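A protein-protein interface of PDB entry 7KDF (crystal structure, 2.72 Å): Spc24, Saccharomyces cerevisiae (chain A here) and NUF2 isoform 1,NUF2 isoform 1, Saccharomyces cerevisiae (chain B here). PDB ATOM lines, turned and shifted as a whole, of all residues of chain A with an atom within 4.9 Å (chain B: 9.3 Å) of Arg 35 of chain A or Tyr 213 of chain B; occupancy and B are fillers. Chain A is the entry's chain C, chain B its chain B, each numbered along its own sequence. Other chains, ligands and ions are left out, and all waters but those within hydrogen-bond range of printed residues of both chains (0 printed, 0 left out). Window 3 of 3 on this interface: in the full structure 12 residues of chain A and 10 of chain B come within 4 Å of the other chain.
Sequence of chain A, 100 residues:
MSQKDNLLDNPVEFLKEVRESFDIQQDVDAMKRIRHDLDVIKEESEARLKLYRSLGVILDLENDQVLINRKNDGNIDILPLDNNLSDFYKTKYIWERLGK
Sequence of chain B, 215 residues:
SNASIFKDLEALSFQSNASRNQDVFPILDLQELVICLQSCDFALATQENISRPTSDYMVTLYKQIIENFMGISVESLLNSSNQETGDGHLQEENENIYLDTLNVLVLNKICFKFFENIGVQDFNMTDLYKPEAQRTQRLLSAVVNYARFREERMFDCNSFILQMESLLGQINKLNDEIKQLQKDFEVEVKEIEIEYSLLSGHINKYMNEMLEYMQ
NH2 of Arg 35 of chain A lies within hydrogen-bond range of O of Tyr 213 of chain B, 2.6 Å away.
Among the printed residues, merely in contact across the chains: Val 28 of chain A with Glu 209 of chain B, Val 28 of chain A with Met 210 of chain B, Val 28 of chain A with Tyr 213 of chain B, Met 31 of chain A with Met 210 of chain B, Met 31 of chain A with Tyr 213 of chain B and Lys 32 of chain A with Tyr 213 of chain B.
Arg 35 of chain A touches just one residue of chain B: Tyr 213. Lys 32 of chain A touches one residue of chain B. Of the printed residues of chain B, Val 28 of chain A touches Glu 209, Met 210 and Tyr 213. Printed residues of chain A within 4 Å of Met 210 of chain B: Val 28 (3.8 Å) and Met 31 (3.6 Å). Met 214 of chain B touches none of the printed residues of chain A. Tyr 206 of chain B touches none of the printed residues of chain A. The nearest printed residue of chain A that does not touch Glu 209 of chain B is Met 31 of chain A (6.7 Å).
Of the 10 printed residues of chain A, 4 touch a printed residue of chain B. Hydrophobic or aromatic side chains of chain A within 4 Å of the printed part of chain B: Val 28 and Met 31. Along chain A the printed residues that touch a printed residue of chain B span positions 28 to 35. Among the printed residues, 7 pairs touch across the chains.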
ATOM      1  N   VAL A  28      -8.589  19.825 -13.346  1.00  0.00           N
ATOM      2  CA  VAL A  28      -8.447  20.829 -14.398  1.00  0.00           C
ATOM      3  C   VAL A  28      -9.664  20.809 -15.312  1.00  0.00           C
ATOM      4  O   VAL A  28     -10.215  21.861 -15.666  1.00  0.00           O
ATOM      5  CB  VAL A  28      -7.143  20.606 -15.187  1.00  0.00           C
ATOM      6  CG1 VAL A  28      -7.175  21.393 -16.491  1.00  0.00           C
ATOM      7  CG2 VAL A  28      -5.945  21.013 -14.351  1.00  0.00           C
ATOM      8  N   MET A  31     -12.433  22.573 -13.808  1.00  0.00           N
ATOM      9  CA  MET A  31     -12.298  24.025 -13.921  1.00  0.00           C
ATOM     10  C   MET A  31     -12.752  24.518 -15.285  1.00  0.00           C
ATOM     11  O   MET A  31     -13.342  25.601 -15.405  1.00  0.00           O
ATOM     12  CB  MET A  31     -10.853  24.446 -13.661  1.00  0.00           C
ATOM     13  CG  MET A  31     -10.475  24.460 -12.187  1.00  0.00           C
ATOM     14  SD  MET A  31     -11.342  25.748 -11.263  1.00  0.00           S
ATOM     15  CE  MET A  31     -10.996  27.184 -12.271  1.00  0.00           C
ATOM     16  N   LYS A  32     -12.476  23.737 -16.326  1.00  0.00           N
ATOM     17  CA  LYS A  32     -12.917  24.078 -17.673  1.00  0.00           C
ATOM     18  C   LYS A  32     -14.436  24.135 -17.759  1.00  0.00           C
ATOM     19  O   LYS A  32     -15.004  25.071 -18.340  1.00  0.00           O
ATOM     20  CB  LYS A  32     -12.341  23.054 -18.643  1.00  0.00           C
ATOM     21  CG  LYS A  32     -10.845  23.151 -18.785  1.00  0.00           C
ATOM     22  CD  LYS A  32     -10.362  22.063 -19.678  1.00  0.00           C
ATOM     23  CE  LYS A  32      -8.855  22.100 -19.836  1.00  0.00           C
ATOM     24  NZ  LYS A  32      -8.385  21.026 -20.787  1.00  0.00           N
ATOM     25  N   ARG A  33     -15.106  23.151 -17.156  1.00  0.00           N
ATOM     26  CA  ARG A  33     -16.562  23.113 -17.133  1.00  0.00           C
ATOM     27  C   ARG A  33     -17.131  24.273 -16.324  1.00  0.00           C
ATOM     28  O   ARG A  33     -18.137  24.876 -16.715  1.00  0.00           O
ATOM     29  CB  ARG A  33     -17.016  21.768 -16.571  1.00  0.00           C
ATOM     30  CG  ARG A  33     -16.430  20.572 -17.313  1.00  0.00           C
ATOM     31  CD  ARG A  33     -17.246  19.321 -17.068  1.00  0.00           C
ATOM     32  NE  ARG A  33     -17.304  18.991 -15.650  1.00  0.00           N
ATOM     33  CZ  ARG A  33     -16.391  18.269 -15.008  1.00  0.00           C
ATOM     34  NH1 ARG A  33     -15.338  17.788 -15.652  1.00  0.00           N
ATOM     35  NH2 ARG A  33     -16.536  18.030 -13.718  1.00  0.00           N
ATOM     36  N   ILE A  34     -16.494  24.607 -15.199  1.00  0.00           N
ATOM     37  CA  ILE A  34     -16.946  25.748 -14.409  1.00  0.00           C
ATOM     38  C   ILE A  34     -16.809  27.037 -15.211  1.00  0.00           C
ATOM     39  O   ILE A  34     -17.740  27.847 -15.277  1.00  0.00           O
ATOM     40  CB  ILE A  34     -16.184  25.816 -13.074  1.00  0.00           C
ATOM     41  CG1 ILE A  34     -16.364  24.510 -12.299  1.00  0.00           C
ATOM     42  CG2 ILE A  34     -16.655  26.999 -12.257  1.00  0.00           C
ATOM     43  CD1 ILE A  34     -15.576  24.452 -11.016  1.00  0.00           C
ATOM     44  N   ARG A  35     -15.660  27.230 -15.860  1.00  0.00           N
ATOM     45  CA  ARG A  35     -15.493  28.403 -16.712  1.00  0.00           C
ATOM     46  C   ARG A  35     -16.517  28.404 -17.834  1.00  0.00           C
ATOM     47  O   ARG A  35     -17.062  29.457 -18.191  1.00  0.00           O
ATOM     48  CB  ARG A  35     -14.076  28.447 -17.281  1.00  0.00           C
ATOM     49  CG  ARG A  35     -13.752  29.698 -18.094  1.00  0.00           C
ATOM     50  CD  ARG A  35     -14.120  30.996 -17.363  1.00  0.00           C
ATOM     51  NE  ARG A  35     -13.538  31.097 -16.021  1.00  0.00           N
ATOM     52  CZ  ARG A  35     -12.234  31.104 -15.744  1.00  0.00           C
ATOM     53  NH1 ARG A  35     -11.326  31.026 -16.711  1.00  0.00           N
ATOM     54  NH2 ARG A  35     -11.833  31.199 -14.483  1.00  0.00           N
ATOM     55  N   HIS A  36     -16.792  27.229 -18.403  1.00  0.00           N
ATOM     56  CA  HIS A  36     -17.813  27.124 -19.439  1.00  0.00           C
ATOM     57  C   HIS A  36     -19.178  27.528 -18.900  1.00  0.00           C
ATOM     58  O   HIS A  36     -19.909  28.297 -19.535  1.00  0.00           O
ATOM     59  CB  HIS A  36     -17.847  25.699 -19.993  1.00  0.00           C
ATOM     60  CG  HIS A  36     -18.979  25.448 -20.936  1.00  0.00           C
ATOM     61  ND1 HIS A  36     -18.927  25.792 -22.269  1.00  0.00           N
ATOM     62  CD2 HIS A  36     -20.203  24.904 -20.736  1.00  0.00           C
ATOM     63  CE1 HIS A  36     -20.067  25.465 -22.851  1.00  0.00           C
ATOM     64  NE2 HIS A  36     -20.858  24.925 -21.942  1.00  0.00           N
ATOM     65  N   ASP A  37     -19.524  27.038 -17.706  1.00  0.00           N
ATOM     66  CA  ASP A  37     -20.817  27.362 -17.116  1.00  0.00           C
ATOM     67  C   ASP A  37     -20.946  28.856 -16.857  1.00  0.00           C
ATOM     68  O   ASP A  37     -22.023  29.433 -17.043  1.00  0.00           O
ATOM     69  CB  ASP A  37     -21.022  26.561 -15.828  1.00  0.00           C
ATOM     70  CG  ASP A  37     -21.120  25.060 -16.082  1.00  0.00           C
ATOM     71  OD1 ASP A  37     -21.315  24.666 -17.255  1.00  0.00           O
ATOM     72  OD2 ASP A  37     -20.993  24.271 -15.115  1.00  0.00           O
ATOM     73  N   LEU A  38     -19.854  29.502 -16.434  1.00  0.00           N
ATOM     74  CA  LEU A  38     -19.883  30.950 -16.239  1.00  0.00           C
ATOM     75  C   LEU A  38     -20.156  31.677 -17.548  1.00  0.00           C
ATOM     76  O   LEU A  38     -20.942  32.633 -17.584  1.00  0.00           O
ATOM     77  CB  LEU A  38     -18.567  31.426 -15.630  1.00  0.00           C
ATOM     78  CG  LEU A  38     -18.297  30.963 -14.200  1.00  0.00           C
ATOM     79  CD1 LEU A  38     -16.907  31.374 -13.765  1.00  0.00           C
ATOM     80  CD2 LEU A  38     -19.344  31.526 -13.264  1.00  0.00           C
ATOM     81  N   ASP A  39     -19.519  31.241 -18.636  1.00  0.00           N
ATOM     82  CA  ASP A  39     -19.797  31.844 -19.933  1.00  0.00           C
ATOM     83  C   ASP A  39     -21.257  31.651 -20.315  1.00  0.00           C
ATOM     84  O   ASP A  39     -21.894  32.564 -20.858  1.00  0.00           O
ATOM     85  CB  ASP A  39     -18.880  31.248 -20.999  1.00  0.00           C
ATOM     86  CG  ASP A  39     -17.419  31.565 -20.755  1.00  0.00           C
ATOM     87  OD1 ASP A  39     -17.095  32.095 -19.673  1.00  0.00           O
ATOM     88  OD2 ASP A  39     -16.591  31.277 -21.647  1.00  0.00           O
ATOM     89  N   TYR B 206       0.316  20.507 -10.406  1.00  0.00           N
ATOM     90  CA  TYR B 206      -1.133  20.633 -10.238  1.00  0.00           C
ATOM     91  C   TYR B 206      -1.573  22.082 -10.029  1.00  0.00           C
ATOM     92  O   TYR B 206      -2.505  22.563 -10.683  1.00  0.00           O
ATOM     93  CB  TYR B 206      -1.560  19.765  -9.054  1.00  0.00           C
ATOM     94  CG  TYR B 206      -2.994  19.909  -8.615  1.00  0.00           C
ATOM     95  CD1 TYR B 206      -4.027  19.386  -9.379  1.00  0.00           C
ATOM     96  CD2 TYR B 206      -3.313  20.542  -7.423  1.00  0.00           C
ATOM     97  CE1 TYR B 206      -5.340  19.500  -8.977  1.00  0.00           C
ATOM     98  CE2 TYR B 206      -4.624  20.664  -7.012  1.00  0.00           C
ATOM     99  CZ  TYR B 206      -5.635  20.142  -7.794  1.00  0.00           C
ATOM    100  OH  TYR B 206      -6.946  20.262  -7.393  1.00  0.00           O
ATOM    101  N   MET B 207      -0.919  22.793  -9.110  1.00  0.00           N
ATOM    102  CA  MET B 207      -1.297  24.179  -8.855  1.00  0.00           C
ATOM    103  C   MET B 207      -1.062  25.049 -10.083  1.00  0.00           C
ATOM    104  O   MET B 207      -1.866  25.935 -10.388  1.00  0.00           O
ATOM    105  CB  MET B 207      -0.517  24.717  -7.660  1.00  0.00           C
ATOM    106  CG  MET B 207      -0.947  24.120  -6.350  1.00  0.00           C
ATOM    107  SD  MET B 207       0.313  24.394  -5.098  1.00  0.00           S
ATOM    108  CE  MET B 207      -0.718  24.665  -3.689  1.00  0.00           C
ATOM    109  N   ASN B 208       0.034  24.805 -10.805  1.00  0.00           N
ATOM    110  CA  ASN B 208       0.346  25.636 -11.963  1.00  0.00           C
ATOM    111  C   ASN B 208      -0.732  25.522 -13.035  1.00  0.00           C
ATOM    112  O   ASN B 208      -1.145  26.532 -13.617  1.00  0.00           O
ATOM    113  CB  ASN B 208       1.716  25.259 -12.527  1.00  0.00           C
ATOM    114  CG  ASN B 208       2.848  25.555 -11.559  1.00  0.00           C
ATOM    115  OD1 ASN B 208       2.744  26.451 -10.716  1.00  0.00           O
ATOM    116  ND2 ASN B 208       3.937  24.799 -11.671  1.00  0.00           N
ATOM    117  N   GLU B 209      -1.208  24.302 -13.304  1.00  0.00           N
ATOM    118  CA  GLU B 209      -2.283  24.134 -14.276  1.00  0.00           C
ATOM    119  C   GLU B 209      -3.586  24.756 -13.780  1.00  0.00           C
ATOM    120  O   GLU B 209      -4.319  25.377 -14.560  1.00  0.00           O
ATOM    121  CB  GLU B 209      -2.478  22.653 -14.595  1.00  0.00           C
ATOM    122  CG  GLU B 209      -1.215  21.952 -15.068  1.00  0.00           C
ATOM    123  CD  GLU B 209      -1.501  20.791 -16.006  1.00  0.00           C
ATOM    124  OE1 GLU B 209      -2.643  20.698 -16.510  1.00  0.00           O
ATOM    125  OE2 GLU B 209      -0.582  19.973 -16.235  1.00  0.00           O
ATOM    126  N   MET B 210      -3.891  24.603 -12.487  1.00  0.00           N
ATOM    127  CA  MET B 210      -5.127  25.164 -11.948  1.00  0.00           C
ATOM    128  C   MET B 210      -5.113  26.689 -11.954  1.00  0.00           C
ATOM    129  O   MET B 210      -6.166  27.311 -12.135  1.00  0.00           O
ATOM    130  CB  MET B 210      -5.370  24.645 -10.530  1.00  0.00           C
ATOM    131  CG  MET B 210      -5.601  23.142 -10.422  1.00  0.00           C
ATOM    132  SD  MET B 210      -7.161  22.587 -11.132  1.00  0.00           S
ATOM    133  CE  MET B 210      -8.274  22.919  -9.768  1.00  0.00           C
ATOM    134  N   LEU B 211      -3.946  27.308 -11.749  1.00  0.00           N
ATOM    135  CA  LEU B 211      -3.857  28.766 -11.830  1.00  0.00           C
ATOM    136  C   LEU B 211      -4.212  29.297 -13.212  1.00  0.00           C
ATOM    137  O   LEU B 211      -4.699  30.428 -13.325  1.00  0.00           O
ATOM    138  CB  LEU B 211      -2.459  29.249 -11.431  1.00  0.00           C
ATOM    139  CG  LEU B 211      -2.178  29.631  -9.972  1.00  0.00           C
ATOM    140  CD1 LEU B 211      -2.980  30.874  -9.623  1.00  0.00           C
ATOM    141  CD2 LEU B 211      -2.519  28.533  -9.002  1.00  0.00           C
ATOM    142  N   GLU B 212      -3.978  28.513 -14.268  1.00  0.00           N
ATOM    143  CA  GLU B 212      -4.305  28.980 -15.612  1.00  0.00           C
ATOM    144  C   GLU B 212      -5.777  29.349 -15.735  1.00  0.00           C
ATOM    145  O   GLU B 212      -6.129  30.248 -16.507  1.00  0.00           O
ATOM    146  CB  GLU B 212      -3.944  27.913 -16.644  1.00  0.00           C
ATOM    147  CG  GLU B 212      -2.454  27.721 -16.859  1.00  0.00           C
ATOM    148  CD  GLU B 212      -2.153  26.755 -17.988  1.00  0.00           C
ATOM    149  OE1 GLU B 212      -3.005  26.616 -18.893  1.00  0.00           O
ATOM    150  OE2 GLU B 212      -1.072  26.128 -17.966  1.00  0.00           O
ATOM    151  N   TYR B 213      -6.644  28.685 -14.972  1.00  0.00           N
ATOM    152  CA  TYR B 213      -8.084  28.889 -15.044  1.00  0.00           C
ATOM    153  C   TYR B 213      -8.626  29.687 -13.866  1.00  0.00           C
ATOM    154  O   TYR B 213      -9.844  29.733 -13.670  1.00  0.00           O
ATOM    155  CB  TYR B 213      -8.797  27.536 -15.151  1.00  0.00           C
ATOM    156  CG  TYR B 213      -8.315  26.693 -16.313  1.00  0.00           C
ATOM    157  CD1 TYR B 213      -9.020  26.652 -17.505  1.00  0.00           C
ATOM    158  CD2 TYR B 213      -7.151  25.947 -16.220  1.00  0.00           C
ATOM    159  CE1 TYR B 213      -8.579  25.889 -18.571  1.00  0.00           C
ATOM    160  CE2 TYR B 213      -6.706  25.182 -17.278  1.00  0.00           C
ATOM    161  CZ  TYR B 213      -7.423  25.156 -18.448  1.00  0.00           C
ATOM    162  OH  TYR B 213      -6.971  24.399 -19.503  1.00  0.00           O
ATOM    163  N   MET B 214      -7.761  30.320 -13.082  1.00  0.00           N
ATOM    164  CA  MET B 214      -8.175  31.162 -11.970  1.00  0.00           C
ATOM    165  C   MET B 214      -7.815  32.614 -12.259  1.00  0.00           C
ATOM    166  O   MET B 214      -7.166  32.929 -13.261  1.00  0.00           O
ATOM    167  CB  MET B 214      -7.530  30.690 -10.660  1.00  0.00           C
ATOM    168  CG  MET B 214      -8.037  29.333 -10.181  1.00  0.00           C
ATOM    169  SD  MET B 214      -6.867  28.443  -9.131  1.00  0.00           S
ATOM    170  CE  MET B 214      -7.257  29.130  -7.523  1.00  0.00           C
ATOM    171  N   GLN B 215      -8.266  33.498 -11.369  1.00  0.00           N
ATOM    172  CA  GLN B 215      -8.059  34.947 -11.488  1.00  0.00           C
ATOM    173  C   GLN B 215      -8.742  35.526 -12.733  1.00  0.00           C
ATOM    174  O   GLN B 215      -9.150  34.813 -13.650  1.00  0.00           O
ATOM    175  CB  GLN B 215      -6.559  35.281 -11.492  1.00  0.00           C
ATOM    176  CG  GLN B 215      -6.211  36.717 -11.876  1.00  0.00           C
ATOM    177  CD  GLN B 215      -6.874  37.751 -10.983  1.00  0.00           C
ATOM    178  OE1 GLN B 215      -7.473  38.712 -11.468  1.00  0.00           O
ATOM    179  NE2 GLN B 215      -6.766  37.562  -9.673  1.00  0.00           N
ATOM    180  OXT GLN B 215      -8.924  36.740 -12.847  1.00  0.00           O
